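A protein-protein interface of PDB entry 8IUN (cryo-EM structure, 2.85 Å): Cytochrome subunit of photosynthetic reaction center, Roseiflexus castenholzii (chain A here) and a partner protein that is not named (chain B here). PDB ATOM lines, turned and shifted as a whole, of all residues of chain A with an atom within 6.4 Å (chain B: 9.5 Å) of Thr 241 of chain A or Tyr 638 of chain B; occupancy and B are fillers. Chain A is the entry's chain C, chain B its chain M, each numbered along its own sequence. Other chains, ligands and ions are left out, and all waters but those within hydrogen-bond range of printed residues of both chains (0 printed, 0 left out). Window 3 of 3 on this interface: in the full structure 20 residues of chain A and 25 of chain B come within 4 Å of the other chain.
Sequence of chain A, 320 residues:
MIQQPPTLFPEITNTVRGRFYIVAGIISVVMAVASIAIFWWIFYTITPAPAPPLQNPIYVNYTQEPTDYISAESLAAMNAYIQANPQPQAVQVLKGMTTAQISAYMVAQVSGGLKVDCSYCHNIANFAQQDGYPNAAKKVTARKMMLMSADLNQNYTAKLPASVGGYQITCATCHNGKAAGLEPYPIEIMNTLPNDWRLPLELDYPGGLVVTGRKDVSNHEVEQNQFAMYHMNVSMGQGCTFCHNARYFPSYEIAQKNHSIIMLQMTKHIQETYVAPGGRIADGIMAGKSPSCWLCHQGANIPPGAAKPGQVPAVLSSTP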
ATOM      1  N   GLN A 238     -36.370  16.477 -21.094  1.00  0.00           N
ATOM      2  CA  GLN A 238     -35.751  17.754 -20.777  1.00  0.00           C
ATOM      3  C   GLN A 238     -34.982  18.266 -21.988  1.00  0.00           C
ATOM      4  O   GLN A 238     -34.967  17.642 -23.046  1.00  0.00           O
ATOM      5  CB  GLN A 238     -34.811  17.619 -19.573  1.00  0.00           C
ATOM      6  CG  GLN A 238     -35.497  17.285 -18.272  1.00  0.00           C
ATOM      7  CD  GLN A 238     -36.217  18.467 -17.682  1.00  0.00           C
ATOM      8  OE1 GLN A 238     -35.928  19.609 -18.016  1.00  0.00           O
ATOM      9  NE2 GLN A 238     -37.163  18.201 -16.799  1.00  0.00           N
ATOM     10  N   GLY A 239     -34.349  19.425 -21.823  1.00  0.00           N
ATOM     11  CA  GLY A 239     -33.427  19.953 -22.805  1.00  0.00           C
ATOM     12  C   GLY A 239     -31.990  19.645 -22.436  1.00  0.00           C
ATOM     13  O   GLY A 239     -31.698  18.939 -21.471  1.00  0.00           O
ATOM     14  N   CYS A 240     -31.071  20.202 -23.221  1.00  0.00           N
ATOM     15  CA  CYS A 240     -29.659  19.892 -23.029  1.00  0.00           C
ATOM     16  C   CYS A 240     -29.106  20.472 -21.741  1.00  0.00           C
ATOM     17  O   CYS A 240     -28.050  20.029 -21.285  1.00  0.00           O
ATOM     18  CB  CYS A 240     -28.829  20.401 -24.204  1.00  0.00           C
ATOM     19  SG  CYS A 240     -29.265  19.724 -25.799  1.00  0.00           S
ATOM     20  N   THR A 241     -29.759  21.530 -21.259  1.00  0.00           N
ATOM     21  CA  THR A 241     -29.314  22.325 -20.089  1.00  0.00           C
ATOM     22  C   THR A 241     -29.660  21.673 -18.750  1.00  0.00           C
ATOM     23  O   THR A 241     -29.440  22.303 -17.750  1.00  0.00           O
ATOM     24  CB  THR A 241     -29.914  23.726 -20.238  1.00  0.00           C
ATOM     25  OG1 THR A 241     -31.317  23.591 -20.431  1.00  0.00           O
ATOM     26  CG2 THR A 241     -29.302  24.505 -21.377  1.00  0.00           C
ATOM     27  N   PHE A 242     -30.159  20.446 -18.739  1.00  0.00           N
ATOM     28  CA  PHE A 242     -30.492  19.706 -17.507  1.00  0.00           C
ATOM     29  C   PHE A 242     -29.189  19.190 -16.910  1.00  0.00           C
ATOM     30  O   PHE A 242     -29.055  19.232 -15.687  1.00  0.00           O
ATOM     31  CB  PHE A 242     -31.469  18.590 -17.866  1.00  0.00           C
ATOM     32  CG  PHE A 242     -31.985  17.732 -16.738  1.00  0.00           C
ATOM     33  CD1 PHE A 242     -32.829  18.253 -15.773  1.00  0.00           C
ATOM     34  CD2 PHE A 242     -31.667  16.386 -16.668  1.00  0.00           C
ATOM     35  CE1 PHE A 242     -33.321  17.455 -14.753  1.00  0.00           C
ATOM     36  CE2 PHE A 242     -32.151  15.593 -15.642  1.00  0.00           C
ATOM     37  CZ  PHE A 242     -32.981  16.127 -14.690  1.00  0.00           C
ATOM     38  N   CYS A 243     -28.253  18.766 -17.768  1.00  0.00           N
ATOM     39  CA  CYS A 243     -26.947  18.219 -17.341  1.00  0.00           C
ATOM     40  C   CYS A 243     -25.770  19.147 -17.709  1.00  0.00           C
ATOM     41  O   CYS A 243     -24.710  18.885 -17.183  1.00  0.00           O
ATOM     42  CB  CYS A 243     -26.735  16.821 -17.922  1.00  0.00           C
ATOM     43  SG  CYS A 243     -27.958  15.481 -17.698  1.00  0.00           S
ATOM     44  N   HIS A 244     -25.923  20.221 -18.511  1.00  0.00           N
ATOM     45  CA  HIS A 244     -24.829  21.034 -19.015  1.00  0.00           C
ATOM     46  C   HIS A 244     -25.083  22.517 -18.810  1.00  0.00           C
ATOM     47  O   HIS A 244     -26.224  22.973 -18.776  1.00  0.00           O
ATOM     48  CB  HIS A 244     -24.597  20.796 -20.514  1.00  0.00           C
ATOM     49  CG  HIS A 244     -23.968  19.477 -20.830  1.00  0.00           C
ATOM     50  ND1 HIS A 244     -22.620  19.247 -20.685  1.00  0.00           N
ATOM     51  CD2 HIS A 244     -24.502  18.321 -21.284  1.00  0.00           C
ATOM     52  CE1 HIS A 244     -22.350  18.004 -21.031  1.00  0.00           C
ATOM     53  NE2 HIS A 244     -23.474  17.421 -21.401  1.00  0.00           N
ATOM     54  N   ASN A 245     -23.987  23.255 -18.663  1.00  0.00           N
ATOM     55  CA  ASN A 245     -23.943  24.682 -18.952  1.00  0.00           C
ATOM     56  C   ASN A 245     -23.475  24.813 -20.396  1.00  0.00           C
ATOM     57  O   ASN A 245     -22.342  24.458 -20.721  1.00  0.00           O
ATOM     58  CB  ASN A 245     -23.006  25.401 -17.988  1.00  0.00           C
ATOM     59  CG  ASN A 245     -23.154  26.904 -18.029  1.00  0.00           C
ATOM     60  OD1 ASN A 245     -23.484  27.477 -19.055  1.00  0.00           O
ATOM     61  ND2 ASN A 245     -22.905  27.549 -16.905  1.00  0.00           N
ATOM     62  N   ALA A 246     -24.352  25.309 -21.266  1.00  0.00           N
ATOM     63  CA  ALA A 246     -24.124  25.239 -22.700  1.00  0.00           C
ATOM     64  C   ALA A 246     -23.009  26.153 -23.182  1.00  0.00           C
ATOM     65  O   ALA A 246     -22.655  26.085 -24.362  1.00  0.00           O
ATOM     66  CB  ALA A 246     -25.417  25.556 -23.443  1.00  0.00           C
ATOM     67  N   ILE A 254     -23.108  20.932 -12.992  1.00  0.00           N
ATOM     68  CA  ILE A 254     -24.466  20.475 -12.722  1.00  0.00           C
ATOM     69  C   ILE A 254     -24.380  19.019 -12.284  1.00  0.00           C
ATOM     70  O   ILE A 254     -23.718  18.209 -12.940  1.00  0.00           O
ATOM     71  CB  ILE A 254     -25.374  20.629 -13.959  1.00  0.00           C
ATOM     72  CG1 ILE A 254     -25.009  21.880 -14.763  1.00  0.00           C
ATOM     73  CG2 ILE A 254     -26.829  20.672 -13.555  1.00  0.00           C
ATOM     74  CD1 ILE A 254     -25.464  23.172 -14.168  1.00  0.00           C
ATOM     75  N   TRP B 630     -19.571  34.099 -13.112  1.00  0.00           N
ATOM     76  CA  TRP B 630     -20.818  33.350 -12.946  1.00  0.00           C
ATOM     77  C   TRP B 630     -20.721  32.259 -11.881  1.00  0.00           C
ATOM     78  O   TRP B 630     -20.756  31.070 -12.213  1.00  0.00           O
ATOM     79  CB  TRP B 630     -21.246  32.723 -14.275  1.00  0.00           C
ATOM     80  CG  TRP B 630     -22.719  32.717 -14.492  1.00  0.00           C
ATOM     81  CD1 TRP B 630     -23.665  33.227 -13.665  1.00  0.00           C
ATOM     82  CD2 TRP B 630     -23.417  32.179 -15.617  1.00  0.00           C
ATOM     83  NE1 TRP B 630     -24.910  33.043 -14.199  1.00  0.00           N
ATOM     84  CE2 TRP B 630     -24.785  32.397 -15.399  1.00  0.00           C
ATOM     85  CE3 TRP B 630     -23.017  31.529 -16.786  1.00  0.00           C
ATOM     86  CZ2 TRP B 630     -25.757  31.992 -16.309  1.00  0.00           C
ATOM     87  CZ3 TRP B 630     -23.981  31.135 -17.686  1.00  0.00           C
ATOM     88  CH2 TRP B 630     -25.334  31.362 -17.443  1.00  0.00           C
ATOM     89  N   PRO B 633     -25.284  30.564 -10.615  1.00  0.00           N
ATOM     90  CA  PRO B 633     -26.349  30.707 -11.610  1.00  0.00           C
ATOM     91  C   PRO B 633     -27.713  30.342 -11.047  1.00  0.00           C
ATOM     92  O   PRO B 633     -27.841  29.519 -10.138  1.00  0.00           O
ATOM     93  CB  PRO B 633     -25.931  29.732 -12.718  1.00  0.00           C
ATOM     94  CG  PRO B 633     -24.502  29.462 -12.482  1.00  0.00           C
ATOM     95  CD  PRO B 633     -24.312  29.536 -11.008  1.00  0.00           C
ATOM     96  N   ASP B 634     -28.743  30.974 -11.604  1.00  0.00           N
ATOM     97  CA  ASP B 634     -30.139  30.655 -11.304  1.00  0.00           C
ATOM     98  C   ASP B 634     -30.619  29.720 -12.407  1.00  0.00           C
ATOM     99  O   ASP B 634     -31.127  30.153 -13.439  1.00  0.00           O
ATOM    100  CB  ASP B 634     -30.977  31.927 -11.215  1.00  0.00           C
ATOM    101  CG  ASP B 634     -32.472  31.657 -11.215  1.00  0.00           C
ATOM    102  OD1 ASP B 634     -32.961  30.961 -10.304  1.00  0.00           O
ATOM    103  OD2 ASP B 634     -33.163  32.158 -12.123  1.00  0.00           O
ATOM    104  N   TRP B 635     -30.447  28.420 -12.189  1.00  0.00           N
ATOM    105  CA  TRP B 635     -30.674  27.443 -13.243  1.00  0.00           C
ATOM    106  C   TRP B 635     -32.137  27.049 -13.392  1.00  0.00           C
ATOM    107  O   TRP B 635     -32.473  26.330 -14.336  1.00  0.00           O
ATOM    108  CB  TRP B 635     -29.810  26.200 -13.012  1.00  0.00           C
ATOM    109  CG  TRP B 635     -29.264  25.672 -14.291  1.00  0.00           C
ATOM    110  CD1 TRP B 635     -29.569  24.489 -14.889  1.00  0.00           C
ATOM    111  CD2 TRP B 635     -28.346  26.338 -15.160  1.00  0.00           C
ATOM    112  NE1 TRP B 635     -28.886  24.368 -16.072  1.00  0.00           N
ATOM    113  CE2 TRP B 635     -28.130  25.494 -16.261  1.00  0.00           C
ATOM    114  CE3 TRP B 635     -27.682  27.566 -15.111  1.00  0.00           C
ATOM    115  CZ2 TRP B 635     -27.278  25.837 -17.300  1.00  0.00           C
ATOM    116  CZ3 TRP B 635     -26.842  27.902 -16.141  1.00  0.00           C
ATOM    117  CH2 TRP B 635     -26.644  27.043 -17.218  1.00  0.00           C
ATOM    118  N   ALA B 636     -33.016  27.528 -12.512  1.00  0.00           N
ATOM    119  CA  ALA B 636     -34.439  27.246 -12.632  1.00  0.00           C
ATOM    120  C   ALA B 636     -35.041  27.779 -13.921  1.00  0.00           C
ATOM    121  O   ALA B 636     -36.111  27.313 -14.320  1.00  0.00           O
ATOM    122  CB  ALA B 636     -35.189  27.830 -11.438  1.00  0.00           C
ATOM    123  N   GLN B 637     -34.388  28.739 -14.577  1.00  0.00           N
ATOM    124  CA  GLN B 637     -34.860  29.205 -15.874  1.00  0.00           C
ATOM    125  C   GLN B 637     -34.688  28.148 -16.954  1.00  0.00           C
ATOM    126  O   GLN B 637     -35.487  28.090 -17.894  1.00  0.00           O
ATOM    127  CB  GLN B 637     -34.120  30.475 -16.281  1.00  0.00           C
ATOM    128  CG  GLN B 637     -34.546  31.006 -17.627  1.00  0.00           C
ATOM    129  CD  GLN B 637     -33.716  32.159 -18.103  1.00  0.00           C
ATOM    130  OE1 GLN B 637     -32.765  32.564 -17.449  1.00  0.00           O
ATOM    131  NE2 GLN B 637     -34.073  32.703 -19.251  1.00  0.00           N
ATOM    132  N   TYR B 638     -33.666  27.305 -16.840  1.00  0.00           N
ATOM    133  CA  TYR B 638     -33.258  26.430 -17.928  1.00  0.00           C
ATOM    134  C   TYR B 638     -33.737  24.997 -17.761  1.00  0.00           C
ATOM    135  O   TYR B 638     -33.286  24.120 -18.500  1.00  0.00           O
ATOM    136  CB  TYR B 638     -31.738  26.456 -18.076  1.00  0.00           C
ATOM    137  CG  TYR B 638     -31.180  27.818 -18.399  1.00  0.00           C
ATOM    138  CD1 TYR B 638     -31.479  28.442 -19.596  1.00  0.00           C
ATOM    139  CD2 TYR B 638     -30.352  28.479 -17.510  1.00  0.00           C
ATOM    140  CE1 TYR B 638     -30.979  29.682 -19.894  1.00  0.00           C
ATOM    141  CE2 TYR B 638     -29.841  29.718 -17.805  1.00  0.00           C
ATOM    142  CZ  TYR B 638     -30.157  30.314 -19.000  1.00  0.00           C
ATOM    143  OH  TYR B 638     -29.652  31.551 -19.305  1.00  0.00           O
ATOM    144  N   VAL B 639     -34.633  24.733 -16.816  1.00  0.00           N
ATOM    145  CA  VAL B 639     -35.159  23.394 -16.574  1.00  0.00           C
ATOM    146  C   VAL B 639     -36.679  23.461 -16.595  1.00  0.00           C
ATOM    147  O   VAL B 639     -37.273  24.352 -15.979  1.00  0.00           O
ATOM    148  CB  VAL B 639     -34.649  22.818 -15.240  1.00  0.00           C
ATOM    149  CG1 VAL B 639     -35.306  21.490 -14.945  1.00  0.00           C
ATOM    150  CG2 VAL B 639     -33.149  22.651 -15.281  1.00  0.00           C
ATOM    151  N   PHE B 640     -37.304  22.531 -17.312  1.00  0.00           N
ATOM    152  CA  PHE B 640     -38.760  22.424 -17.334  1.00  0.00           C
ATOM    153  C   PHE B 640     -39.266  21.774 -16.052  1.00  0.00           C
ATOM    154  O   PHE B 640     -40.420  21.949 -15.667  1.00  0.00           O
ATOM    155  CB  PHE B 640     -39.234  21.618 -18.545  1.00  0.00           C
ATOM    156  CG  PHE B 640     -38.732  22.138 -19.858  1.00  0.00           C
ATOM    157  CD1 PHE B 640     -39.223  23.314 -20.387  1.00  0.00           C
ATOM    158  CD2 PHE B 640     -37.778  21.442 -20.571  1.00  0.00           C
ATOM    159  CE1 PHE B 640     -38.760  23.786 -21.595  1.00  0.00           C
ATOM    160  CE2 PHE B 640     -37.318  21.914 -21.772  1.00  0.00           C
ATOM    161  CZ  PHE B 640     -37.808  23.084 -22.284  1.00  0.00           C
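Among the printed residues, pairs that only touch across the chains: His 244 of chain A with Trp 635 of chain B (3.4 Å), Asn 245 of chain A with Trp 635 of chain B (3.6 Å), Gln 238 of chain A with Val 639 of chain B (3.7 Å), Asn 245 of chain A with Trp 630 of chain B (3.8 Å) and Gly 239 of chain A with Phe 640 of chain B (3.9 Å).
Of the 10 printed residues of chain A, 5 touch a printed residue of chain B. Hydrophobic or aromatic side chains of chain B within 4 Å of the printed part of chain A: Trp 630, Trp 635, Tyr 638, Val 639 and Phe 640. Among the printed residues, 8 pairs touch across the chains. Among the printed residues, no Asp or Glu carboxylate lies within 4 Å of a Lys or Arg side-chain nitrogen of the other chain.
The indole nitrogen of Trp 635 of chain B is in hydrogen-bond range of the backbone carbonyl oxygen of Thr 241 of chain A (2.7 Å). The side-chain amide oxygen (OE1) of Gln 238 of chain A lies within hydrogen-bond range of the backbone NH (N) of Phe 640 of chain B (3.3 Å). The backbone carbonyl oxygen (O) of Tyr 638 of chain B sits at hydrogen-bond distance from the side-chain hydroxyl (OG1) of Thr 241 of chain A (2.8 Å).
Of chain B, only Trp 635 and Tyr 638 come within 4 Å of Thr 241 of chain A. Of chain A, only Thr 241 (2.8 Å) comes within 4 Å of Tyr 638 of chain B. Gly 239 of chain A touches one residue of chain B. Printed residues of chain B within 4 Å of Asn 245 of chain A: Trp 630 and Trp 635. Of the printed residues of chain A, Trp 635 of chain B touches Thr 241, His 244 and Asn 245. Of the printed residues of chain A, Phe 640 of chain B touches Gln 238 (3.3 Å) and Gly 239 (3.9 Å). Printed residues of chain A within 4 Å of Trp 630 of chain B: Asn 245 (3.8 Å). Printed residues of chain A within 4 Å of Val 639 of chain B: Gln 238 (3.7 Å). Pro 633 of chain B touches none of the printed residues of chain A. Gln 637 of chain B touches none of the printed residues of chain A. The nearest residue of chain B that does not touch Thr 241 of chain A is Val 639 of chain B (4.5 Å).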
